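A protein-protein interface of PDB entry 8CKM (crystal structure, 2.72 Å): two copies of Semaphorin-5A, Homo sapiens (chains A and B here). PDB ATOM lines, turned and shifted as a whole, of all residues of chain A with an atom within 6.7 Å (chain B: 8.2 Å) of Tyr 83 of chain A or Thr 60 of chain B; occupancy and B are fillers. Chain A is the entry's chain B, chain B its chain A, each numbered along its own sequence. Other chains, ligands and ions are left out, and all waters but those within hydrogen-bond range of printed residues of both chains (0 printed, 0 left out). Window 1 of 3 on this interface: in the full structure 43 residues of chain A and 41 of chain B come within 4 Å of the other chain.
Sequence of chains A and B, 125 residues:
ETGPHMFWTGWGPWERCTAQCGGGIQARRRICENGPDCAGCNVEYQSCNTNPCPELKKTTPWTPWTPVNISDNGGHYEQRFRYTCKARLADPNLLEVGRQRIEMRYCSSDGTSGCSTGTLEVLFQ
O of Pro 61 of chain B is in hydrogen-bond range of OH of Tyr 83 of chain A (2.8 Å). OH of Tyr 83 of chain A is in hydrogen-bond range of O of Trp 62 of chain B, at 3.4 Å. The side-chain hydroxyl (OH) of Tyr 83 of chain B sits at hydrogen-bond distance from the backbone carbonyl oxygen (O) of Pro 61 of chain A (2.7 Å). SG of Cys 85 of chain B forms a disulfide with SG of Cys 85 of chain A (2.0 Å). N of Gly 98 of chain B sits at hydrogen-bond distance from O of Thr 84 of chain A, 2.7 Å away. OH of Tyr 83 of chain A is in hydrogen-bond range of NE2 of Gln 100 of chain B, at 3.2 Å. N of Arg 101 of chain B sits at hydrogen-bond distance from O of Arg 82 of chain A, at 2.8 Å.
O of Lys 58 of chain B is in hydrogen-bond range of N of Cys 85 of chain B (2.6 Å). N of Thr 60 of chain B lies within hydrogen-bond range of O of Tyr 83 of chain B (2.7 Å). N of Phe 81 of chain B sits at hydrogen-bond distance from OG1 of Thr 63 of chain B (2.7 Å). The backbone NH (N) of Cys 85 of chain A lies within hydrogen-bond range of the backbone carbonyl oxygen (O) of Lys 58 of chain A (2.7 Å). The backbone NH (N) of Tyr 83 of chain A lies within hydrogen-bond range of the side-chain hydroxyl (OG1) of Thr 60 of chain A, 2.6 Å away. N of Phe 81 of chain A is in hydrogen-bond range of OG1 of Thr 63 of chain A, at 2.5 Å.
CG2 of Thr 63 of chain A touches CD1 of Phe 81 of chain B, 3.6 Å away. Thr 63 of chain B touches Phe 81 of chain A. Pro 64 of chain B touches Phe 81 of chain A (CD to CE2, 3.8 Å). Gln 100 of chain B touches Phe 81 of chain A. Arg 82 of chain A touches Gln 100 of chain B. Thr 63 of chain B touches Tyr 83 of chain A (N to OH, 3.8 Å). Tyr 83 of chain A touches Arg 99 of chain B (CA to O, 3.9 Å). Val 97 of chain B touches Thr 84 of chain A. Thr 84 of chain A touches Arg 101 of chain B. O of Thr 84 of chain B touches C of Val 97 of chain A, at 3.4 Å.
Of the printed residues of chain B, Tyr 83 of chain A touches Thr 60, Pro 61, Trp 62, Thr 63, Gly 98, Arg 99 and Gln 100. Printed residues of chain A within 4 Å of Val 97 of chain B: Thr 84 (3.5 Å). Of the printed residues of chain B, Cys 85 of chain A touches Cys 85 (2.0 Å) and Glu 96 (3.9 Å). Lys 58 of chain A touches none of the printed residues of chain B. Thr 59 of chain B touches none of the printed residues of chain A. The nearest residue of chain B that does not touch Tyr 83 of chain A is Val 97 of chain B (4.2 Å).
Of the 20 printed residues of chain B, 16 touch a printed residue of chain A. Along chain A the printed residues that touch a printed residue of chain B span positions 61 to 97. Among the printed residues, 24 pairs touch across the chains.
Pro 61 of chain A touches Tyr 83 of chain B, and with the chains exchanged Tyr 83 of chain A touches Pro 61 of chain B. Thr 63 of chain A touches Tyr 83 of chain B, and with the chains exchanged Tyr 83 of chain A touches Thr 63 of chain B. Tyr 83 of chain A touches Thr 60 of chain B, but with the chains exchanged Thr 60 of chain A does not touch Tyr 83 of chain B (4.04 Å). Thr 84 of chain A touches Val 97 of chain B, and with the chains exchanged Val 97 of chain A touches Thr 84 of chain B. Of the 24 pairs that touch across the chains among the printed residues, 9 have their exchanged pair printed and touching as well.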
ATOM      1  N   LYS A  58     -22.572  38.079 -13.887  1.00  0.00           N
ATOM      2  CA  LYS A  58     -21.294  37.679 -13.318  1.00  0.00           C
ATOM      3  C   LYS A  58     -21.108  36.183 -13.518  1.00  0.00           C
ATOM      4  O   LYS A  58     -22.074  35.415 -13.474  1.00  0.00           O
ATOM      5  CB  LYS A  58     -21.202  38.044 -11.829  1.00  0.00           C
ATOM      6  CG  LYS A  58     -21.149  39.545 -11.573  1.00  0.00           C
ATOM      7  CD  LYS A  58     -20.988  39.868 -10.094  1.00  0.00           C
ATOM      8  CE  LYS A  58     -20.952  41.374  -9.867  1.00  0.00           C
ATOM      9  NZ  LYS A  58     -20.902  41.737  -8.424  1.00  0.00           N
ATOM     10  N   THR A  59     -19.863  35.777 -13.743  1.00  0.00           N
ATOM     11  CA  THR A  59     -19.540  34.391 -14.051  1.00  0.00           C
ATOM     12  C   THR A  59     -19.103  33.650 -12.796  1.00  0.00           C
ATOM     13  O   THR A  59     -18.366  34.188 -11.966  1.00  0.00           O
ATOM     14  CB  THR A  59     -18.428  34.315 -15.096  1.00  0.00           C
ATOM     15  OG1 THR A  59     -17.251  34.955 -14.586  1.00  0.00           O
ATOM     16  CG2 THR A  59     -18.858  35.001 -16.383  1.00  0.00           C
ATOM     17  N   THR A  60     -19.568  32.412 -12.664  1.00  0.00           N
ATOM     18  CA  THR A  60     -19.091  31.550 -11.599  1.00  0.00           C
ATOM     19  C   THR A  60     -17.675  31.073 -11.907  1.00  0.00           C
ATOM     20  O   THR A  60     -17.251  31.058 -13.067  1.00  0.00           O
ATOM     21  CB  THR A  60     -20.018  30.351 -11.421  1.00  0.00           C
ATOM     22  OG1 THR A  60     -19.970  29.528 -12.592  1.00  0.00           O
ATOM     23  CG2 THR A  60     -21.446  30.816 -11.185  1.00  0.00           C
ATOM     24  N   PRO A  61     -16.911  30.703 -10.879  1.00  0.00           N
ATOM     25  CA  PRO A  61     -15.582  30.135 -11.123  1.00  0.00           C
ATOM     26  C   PRO A  61     -15.674  28.817 -11.872  1.00  0.00           C
ATOM     27  O   PRO A  61     -16.638  28.060 -11.733  1.00  0.00           O
ATOM     28  CB  PRO A  61     -15.016  29.936  -9.714  1.00  0.00           C
ATOM     29  CG  PRO A  61     -15.760  30.908  -8.870  1.00  0.00           C
ATOM     30  CD  PRO A  61     -17.143  30.953  -9.447  1.00  0.00           C
ATOM     31  N   THR A  63     -15.088  25.021 -12.824  1.00  0.00           N
ATOM     32  CA  THR A  63     -14.823  23.756 -12.168  1.00  0.00           C
ATOM     33  C   THR A  63     -13.467  23.224 -12.624  1.00  0.00           C
ATOM     34  O   THR A  63     -12.981  23.587 -13.696  1.00  0.00           O
ATOM     35  CB  THR A  63     -15.924  22.749 -12.491  1.00  0.00           C
ATOM     36  OG1 THR A  63     -16.034  22.592 -13.912  1.00  0.00           O
ATOM     37  CG2 THR A  63     -17.255  23.221 -11.928  1.00  0.00           C
ATOM     38  N   PHE A  81     -16.905  23.185 -16.231  1.00  0.00           N
ATOM     39  CA  PHE A  81     -18.227  23.793 -16.273  1.00  0.00           C
ATOM     40  C   PHE A  81     -18.285  25.056 -15.424  1.00  0.00           C
ATOM     41  O   PHE A  81     -17.537  25.216 -14.456  1.00  0.00           O
ATOM     42  CB  PHE A  81     -19.311  22.811 -15.793  1.00  0.00           C
ATOM     43  CG  PHE A  81     -19.244  21.457 -16.444  1.00  0.00           C
ATOM     44  CD1 PHE A  81     -18.370  20.491 -15.971  1.00  0.00           C
ATOM     45  CD2 PHE A  81     -20.060  21.147 -17.518  1.00  0.00           C
ATOM     46  CE1 PHE A  81     -18.298  19.249 -16.564  1.00  0.00           C
ATOM     47  CE2 PHE A  81     -19.997  19.901 -18.113  1.00  0.00           C
ATOM     48  CZ  PHE A  81     -19.114  18.950 -17.634  1.00  0.00           C
ATOM     49  N   ARG A  82     -19.192  25.954 -15.804  1.00  0.00           N
ATOM     50  CA  ARG A  82     -19.461  27.166 -15.043  1.00  0.00           C
ATOM     51  C   ARG A  82     -20.831  27.694 -15.441  1.00  0.00           C
ATOM     52  O   ARG A  82     -21.402  27.293 -16.459  1.00  0.00           O
ATOM     53  CB  ARG A  82     -18.386  28.234 -15.267  1.00  0.00           C
ATOM     54  CG  ARG A  82     -18.449  28.901 -16.628  1.00  0.00           C
ATOM     55  CD  ARG A  82     -17.506  30.091 -16.700  1.00  0.00           C
ATOM     56  NE  ARG A  82     -17.548  30.732 -18.010  1.00  0.00           N
ATOM     57  CZ  ARG A  82     -16.791  31.760 -18.365  1.00  0.00           C
ATOM     58  NH1 ARG A  82     -15.915  32.295 -17.531  1.00  0.00           N
ATOM     59  NH2 ARG A  82     -16.914  32.261 -19.592  1.00  0.00           N
ATOM     60  N   TYR A  83     -21.351  28.603 -14.622  1.00  0.00           N
ATOM     61  CA  TYR A  83     -22.652  29.211 -14.850  1.00  0.00           C
ATOM     62  C   TYR A  83     -22.521  30.724 -14.738  1.00  0.00           C
ATOM     63  O   TYR A  83     -21.455  31.260 -14.420  1.00  0.00           O
ATOM     64  CB  TYR A  83     -23.702  28.690 -13.854  1.00  0.00           C
ATOM     65  CG  TYR A  83     -23.947  27.193 -13.907  1.00  0.00           C
ATOM     66  CD1 TYR A  83     -23.053  26.298 -13.326  1.00  0.00           C
ATOM     67  CD2 TYR A  83     -25.088  26.677 -14.508  1.00  0.00           C
ATOM     68  CE1 TYR A  83     -23.273  24.937 -13.365  1.00  0.00           C
ATOM     69  CE2 TYR A  83     -25.317  25.314 -14.549  1.00  0.00           C
ATOM     70  CZ  TYR A  83     -24.406  24.450 -13.975  1.00  0.00           C
ATOM     71  OH  TYR A  83     -24.625  23.092 -14.009  1.00  0.00           O
ATOM     72  N   THR A  84     -23.625  31.417 -15.008  1.00  0.00           N
ATOM     73  CA  THR A  84     -23.670  32.871 -14.945  1.00  0.00           C
ATOM     74  C   THR A  84     -24.803  33.298 -14.025  1.00  0.00           C
ATOM     75  O   THR A  84     -25.915  32.766 -14.116  1.00  0.00           O
ATOM     76  CB  THR A  84     -23.865  33.487 -16.336  1.00  0.00           C
ATOM     77  OG1 THR A  84     -25.236  33.361 -16.728  1.00  0.00           O
ATOM     78  CG2 THR A  84     -22.998  32.780 -17.367  1.00  0.00           C
ATOM     79  N   CYS A  85     -24.522  34.252 -13.142  1.00  0.00           N
ATOM     80  CA  CYS A  85     -25.531  34.832 -12.265  1.00  0.00           C
ATOM     81  C   CYS A  85     -25.990  36.154 -12.866  1.00  0.00           C
ATOM     82  O   CYS A  85     -25.173  37.052 -13.096  1.00  0.00           O
ATOM     83  CB  CYS A  85     -24.981  35.044 -10.855  1.00  0.00           C
ATOM     84  SG  CYS A  85     -24.478  33.538  -9.990  1.00  0.00           S
ATOM     85  N   VAL A  97     -21.576  35.704  -6.148  1.00  0.00           N
ATOM     86  CA  VAL A  97     -21.664  34.265  -6.355  1.00  0.00           C
ATOM     87  C   VAL A  97     -21.227  33.575  -5.072  1.00  0.00           C
ATOM     88  O   VAL A  97     -20.190  33.925  -4.492  1.00  0.00           O
ATOM     89  CB  VAL A  97     -20.804  33.822  -7.551  1.00  0.00           C
ATOM     90  CG1 VAL A  97     -20.955  32.327  -7.798  1.00  0.00           C
ATOM     91  CG2 VAL A  97     -21.181  34.614  -8.792  1.00  0.00           C
ATOM     92  N   LYS B  57     -31.235  34.287  -2.790  1.00  0.00           N
ATOM     93  CA  LYS B  57     -30.276  33.336  -3.329  1.00  0.00           C
ATOM     94  C   LYS B  57     -30.980  32.262  -4.145  1.00  0.00           C
ATOM     95  O   LYS B  57     -32.070  31.813  -3.788  1.00  0.00           O
ATOM     96  CB  LYS B  57     -29.454  32.679  -2.208  1.00  0.00           C
ATOM     97  N   LYS B  58     -30.350  31.874  -5.253  1.00  0.00           N
ATOM     98  CA  LYS B  58     -30.771  30.743  -6.065  1.00  0.00           C
ATOM     99  C   LYS B  58     -29.553  29.882  -6.364  1.00  0.00           C
ATOM    100  O   LYS B  58     -28.425  30.380  -6.432  1.00  0.00           O
ATOM    101  CB  LYS B  58     -31.430  31.193  -7.378  1.00  0.00           C
ATOM    102  CG  LYS B  58     -32.757  31.909  -7.202  1.00  0.00           C
ATOM    103  CD  LYS B  58     -33.355  32.279  -8.546  1.00  0.00           C
ATOM    104  CE  LYS B  58     -34.734  32.890  -8.392  1.00  0.00           C
ATOM    105  NZ  LYS B  58     -35.335  33.236  -9.709  1.00  0.00           N
ATOM    106  N   THR B  59     -29.788  28.585  -6.545  1.00  0.00           N
ATOM    107  CA  THR B  59     -28.717  27.620  -6.758  1.00  0.00           C
ATOM    108  C   THR B  59     -28.631  27.237  -8.229  1.00  0.00           C
ATOM    109  O   THR B  59     -29.654  27.011  -8.880  1.00  0.00           O
ATOM    110  CB  THR B  59     -28.949  26.364  -5.918  1.00  0.00           C
ATOM    111  OG1 THR B  59     -30.224  25.798  -6.247  1.00  0.00           O
ATOM    112  CG2 THR B  59     -28.917  26.693  -4.433  1.00  0.00           C
ATOM    113  N   THR B  60     -27.408  27.147  -8.751  1.00  0.00           N
ATOM    114  CA  THR B  60     -27.246  26.653 -10.111  1.00  0.00           C
ATOM    115  C   THR B  60     -27.519  25.151 -10.151  1.00  0.00           C
ATOM    116  O   THR B  60     -27.475  24.474  -9.120  1.00  0.00           O
ATOM    117  CB  THR B  60     -25.842  26.930 -10.651  1.00  0.00           C
ATOM    118  OG1 THR B  60     -24.914  25.982 -10.107  1.00  0.00           O
ATOM    119  CG2 THR B  60     -25.397  28.345 -10.319  1.00  0.00           C
ATOM    120  N   PRO B  61     -27.835  24.612 -11.324  1.00  0.00           N
ATOM    121  CA  PRO B  61     -27.957  23.159 -11.450  1.00  0.00           C
ATOM    122  C   PRO B  61     -26.628  22.471 -11.189  1.00  0.00           C
ATOM    123  O   PRO B  61     -25.553  23.047 -11.372  1.00  0.00           O
ATOM    124  CB  PRO B  61     -28.406  22.965 -12.901  1.00  0.00           C
ATOM    125  CG  PRO B  61     -29.082  24.244 -13.251  1.00  0.00           C
ATOM    126  CD  PRO B  61     -28.317  25.309 -12.528  1.00  0.00           C
ATOM    127  N   TRP B  62     -26.718  21.230 -10.722  1.00  0.00           N
ATOM    128  CA  TRP B  62     -25.525  20.418 -10.533  1.00  0.00           C
ATOM    129  C   TRP B  62     -24.838  20.165 -11.867  1.00  0.00           C
ATOM    130  O   TRP B  62     -25.491  19.970 -12.896  1.00  0.00           O
ATOM    131  CB  TRP B  62     -25.884  19.084  -9.876  1.00  0.00           C
ATOM    132  CG  TRP B  62     -26.179  19.169  -8.407  1.00  0.00           C
ATOM    133  CD1 TRP B  62     -27.403  19.084  -7.809  1.00  0.00           C
ATOM    134  CD2 TRP B  62     -25.227  19.340  -7.351  1.00  0.00           C
ATOM    135  NE1 TRP B  62     -27.272  19.196  -6.444  1.00  0.00           N
ATOM    136  CE2 TRP B  62     -25.946  19.355  -6.139  1.00  0.00           C
ATOM    137  CE3 TRP B  62     -23.837  19.486  -7.314  1.00  0.00           C
ATOM    138  CZ2 TRP B  62     -25.320  19.509  -4.903  1.00  0.00           C
ATOM    139  CZ3 TRP B  62     -23.218  19.639  -6.086  1.00  0.00           C
ATOM    140  CH2 TRP B  62     -23.959  19.649  -4.897  1.00  0.00           C
ATOM    141  N   THR B  63     -23.510  20.182 -11.851  1.00  0.00           N
ATOM    142  CA  THR B  63     -22.754  19.743 -13.006  1.00  0.00           C
ATOM    143  C   THR B  63     -22.903  18.232 -13.161  1.00  0.00           C
ATOM    144  O   THR B  63     -23.227  17.533 -12.200  1.00  0.00           O
ATOM    145  CB  THR B  63     -21.282  20.122 -12.855  1.00  0.00           C
ATOM    146  OG1 THR B  63     -20.769  19.579 -11.632  1.00  0.00           O
ATOM    147  CG2 THR B  63     -21.123  21.633 -12.841  1.00  0.00           C
ATOM    148  N   PRO B  64     -22.696  17.705 -14.367  1.00  0.00           N
ATOM    149  CA  PRO B  64     -22.732  16.249 -14.538  1.00  0.00           C
ATOM    150  C   PRO B  64     -21.652  15.580 -13.701  1.00  0.00           C
ATOM    151  O   PRO B  64     -20.620  16.177 -13.384  1.00  0.00           O
ATOM    152  CB  PRO B  64     -22.480  16.057 -16.038  1.00  0.00           C
ATOM    153  CG  PRO B  64     -22.866  17.355 -16.656  1.00  0.00           C
ATOM    154  CD  PRO B  64     -22.519  18.404 -15.650  1.00  0.00           C
ATOM    155  N   PHE B  81     -20.525  19.683  -8.920  1.00  0.00           N
ATOM    156  CA  PHE B  81     -20.430  20.978  -8.268  1.00  0.00           C
ATOM    157  C   PHE B  81     -21.676  21.804  -8.548  1.00  0.00           C
ATOM    158  O   PHE B  81     -22.355  21.619  -9.563  1.00  0.00           O
ATOM    159  CB  PHE B  81     -19.195  21.763  -8.742  1.00  0.00           C
ATOM    160  CG  PHE B  81     -17.953  20.927  -8.885  1.00  0.00           C
ATOM    161  CD1 PHE B  81     -17.699  20.231 -10.057  1.00  0.00           C
ATOM    162  CD2 PHE B  81     -17.038  20.844  -7.855  1.00  0.00           C
ATOM    163  CE1 PHE B  81     -16.561  19.460 -10.190  1.00  0.00           C
ATOM    164  CE2 PHE B  81     -15.897  20.076  -7.983  1.00  0.00           C
ATOM    165  CZ  PHE B  81     -15.658  19.383  -9.151  1.00  0.00           C
ATOM    166  N   ARG B  82     -21.966  22.730  -7.638  1.00  0.00           N
ATOM    167  CA  ARG B  82     -22.982  23.741  -7.887  1.00  0.00           C
ATOM    168  C   ARG B  82     -22.620  24.997  -7.111  1.00  0.00           C
ATOM    169  O   ARG B  82     -21.816  24.966  -6.174  1.00  0.00           O
ATOM    170  CB  ARG B  82     -24.384  23.251  -7.513  1.00  0.00           C
ATOM    171  CG  ARG B  82     -24.732  23.373  -6.045  1.00  0.00           C
ATOM    172  CD  ARG B  82     -26.222  23.170  -5.829  1.00  0.00           C
ATOM    173  NE  ARG B  82     -26.599  23.314  -4.429  1.00  0.00           N
ATOM    174  CZ  ARG B  82     -27.832  23.161  -3.963  1.00  0.00           C
ATOM    175  NH1 ARG B  82     -28.843  22.862  -4.763  1.00  0.00           N
ATOM    176  NH2 ARG B  82     -28.056  23.311  -2.660  1.00  0.00           N
ATOM    177  N   TYR B  83     -23.209  26.109  -7.532  1.00  0.00           N
ATOM    178  CA  TYR B  83     -22.969  27.414  -6.941  1.00  0.00           C
ATOM    179  C   TYR B  83     -24.300  28.051  -6.576  1.00  0.00           C
ATOM    180  O   TYR B  83     -25.371  27.579  -6.966  1.00  0.00           O
ATOM    181  CB  TYR B  83     -22.203  28.332  -7.902  1.00  0.00           C
ATOM    182  CG  TYR B  83     -20.882  27.795  -8.402  1.00  0.00           C
ATOM    183  CD1 TYR B  83     -20.831  26.905  -9.465  1.00  0.00           C
ATOM    184  CD2 TYR B  83     -19.683  28.201  -7.831  1.00  0.00           C
ATOM    185  CE1 TYR B  83     -19.627  26.418  -9.931  1.00  0.00           C
ATOM    186  CE2 TYR B  83     -18.476  27.721  -8.292  1.00  0.00           C
ATOM    187  CZ  TYR B  83     -18.453  26.830  -9.341  1.00  0.00           C
ATOM    188  OH  TYR B  83     -17.251  26.349  -9.804  1.00  0.00           O
ATOM    189  N   THR B  84     -24.222  29.142  -5.822  1.00  0.00           N
ATOM    190  CA  THR B  84     -25.397  29.892  -5.404  1.00  0.00           C
ATOM    191  C   THR B  84     -25.241  31.344  -5.838  1.00  0.00           C
ATOM    192  O   THR B  84     -24.194  31.957  -5.605  1.00  0.00           O
ATOM    193  CB  THR B  84     -25.599  29.795  -3.888  1.00  0.00           C
ATOM    194  OG1 THR B  84     -24.485  30.392  -3.214  1.00  0.00           O
ATOM    195  CG2 THR B  84     -25.705  28.336  -3.457  1.00  0.00           C
ATOM    196  N   CYS B  85     -26.276  31.883  -6.478  1.00  0.00           N
ATOM    197  CA  CYS B  85     -26.284  33.268  -6.934  1.00  0.00           C
ATOM    198  C   CYS B  85     -26.988  34.132  -5.895  1.00  0.00           C
ATOM    199  O   CYS B  85     -28.197  33.988  -5.680  1.00  0.00           O
ATOM    200  CB  CYS B  85     -26.986  33.393  -8.286  1.00  0.00           C
ATOM    201  SG  CYS B  85     -26.208  32.521  -9.665  1.00  0.00           S
ATOM    202  N   GLU B  96     -31.775  35.306 -11.846  1.00  0.00           N
ATOM    203  CA  GLU B  96     -31.846  34.157 -12.733  1.00  0.00           C
ATOM    204  C   GLU B  96     -30.451  33.588 -12.936  1.00  0.00           C
ATOM    205  O   GLU B  96     -29.452  34.312 -12.886  1.00  0.00           O
ATOM    206  CB  GLU B  96     -32.483  34.539 -14.075  1.00  0.00           C
ATOM    207  CG  GLU B  96     -32.825  33.359 -14.975  1.00  0.00           C
ATOM    208  CD  GLU B  96     -33.725  33.747 -16.130  1.00  0.00           C
ATOM    209  OE1 GLU B  96     -34.527  34.694 -15.973  1.00  0.00           O
ATOM    210  OE2 GLU B  96     -33.631  33.105 -17.197  1.00  0.00           O
ATOM    211  N   VAL B  97     -30.396  32.279 -13.165  1.00  0.00           N
ATOM    212  CA  VAL B  97     -29.149  31.562 -13.386  1.00  0.00           C
ATOM    213  C   VAL B  97     -29.028  31.250 -14.869  1.00  0.00           C
ATOM    214  O   VAL B  97     -29.955  30.700 -15.475  1.00  0.00           O
ATOM    215  CB  VAL B  97     -29.094  30.276 -12.545  1.00  0.00           C
ATOM    216  CG1 VAL B  97     -27.864  29.457 -12.901  1.00  0.00           C
ATOM    217  CG2 VAL B  97     -29.097  30.625 -11.068  1.00  0.00           C
ATOM    218  N   GLY B  98     -27.884  31.597 -15.452  1.00  0.00           N
ATOM    219  CA  GLY B  98     -27.662  31.375 -16.860  1.00  0.00           C
ATOM    220  C   GLY B  98     -27.444  29.914 -17.190  1.00  0.00           C
ATOM    221  O   GLY B  98     -27.468  29.033 -16.331  1.00  0.00           O
ATOM    222  N   ARG B  99     -27.228  29.662 -18.478  1.00  0.00           N
ATOM    223  CA  ARG B  99     -27.017  28.307 -18.956  1.00  0.00           C
ATOM    224  C   ARG B  99     -25.677  27.771 -18.466  1.00  0.00           C
ATOM    225  O   ARG B  99     -24.810  28.509 -17.989  1.00  0.00           O
ATOM    226  CB  ARG B  99     -27.072  28.261 -20.483  1.00  0.00           C
ATOM    227  N   GLN B 100     -25.525  26.456 -18.569  1.00  0.00           N
ATOM    228  CA  GLN B 100     -24.256  25.824 -18.248  1.00  0.00           C
ATOM    229  C   GLN B 100     -23.278  26.006 -19.403  1.00  0.00           C
ATOM    230  O   GLN B 100     -23.621  25.772 -20.565  1.00  0.00           O
ATOM    231  CB  GLN B 100     -24.469  24.340 -17.956  1.00  0.00           C
ATOM    232  CG  GLN B 100     -23.193  23.525 -17.862  1.00  0.00           C
ATOM    233  CD  GLN B 100     -23.462  22.030 -17.847  1.00  0.00           C
ATOM    234  OE1 GLN B 100     -23.066  21.307 -18.761  1.00  0.00           O
ATOM    235  NE2 GLN B 100     -24.136  21.561 -16.804  1.00  0.00           N
ATOM    236  N   ARG B 101     -22.060  26.432 -19.081  1.00  0.00           N
ATOM    237  CA  ARG B 101     -21.004  26.610 -20.066  1.00  0.00           C
ATOM    238  C   ARG B 101     -20.018  25.458 -19.931  1.00  0.00           C
ATOM    239  O   ARG B 101     -19.416  25.276 -18.869  1.00  0.00           O
ATOM    240  CB  ARG B 101     -20.288  27.945 -19.861  1.00  0.00           C
ATOM    241  CG  ARG B 101     -21.195  29.157 -19.724  1.00  0.00           C
ATOM    242  CD  ARG B 101     -21.679  29.641 -21.074  1.00  0.00           C
ATOM    243  NE  ARG B 101     -22.133  31.026 -21.028  1.00  0.00           N
ATOM    244  CZ  ARG B 101     -21.336  32.081 -21.146  1.00  0.00           C
ATOM    245  NH1 ARG B 101     -20.027  31.947 -21.290  1.00  0.00           N
ATOM    246  NH2 ARG B 101     -21.866  33.300 -21.122  1.00  0.00           N
ATOM    247  N   ILE B 102     -19.842  24.693 -21.003  1.00  0.00           N
ATOM    248  CA  ILE B 102     -18.866  23.610 -21.043  1.00  0.00           C
ATOM    249  C   ILE B 102     -17.668  24.072 -21.857  1.00  0.00           C
ATOM    250  O   ILE B 102     -17.829  24.568 -22.977  1.00  0.00           O
ATOM    251  CB  ILE B 102     -19.472  22.331 -21.643  1.00  0.00           C
ATOM    252  CG1 ILE B 102     -20.853  22.057 -21.037  1.00  0.00           C
ATOM    253  CG2 ILE B 102     -18.549  21.145 -21.411  1.00  0.00           C
ATOM    254  CD1 ILE B 102     -21.581  20.900 -21.691  1.00  0.00           C
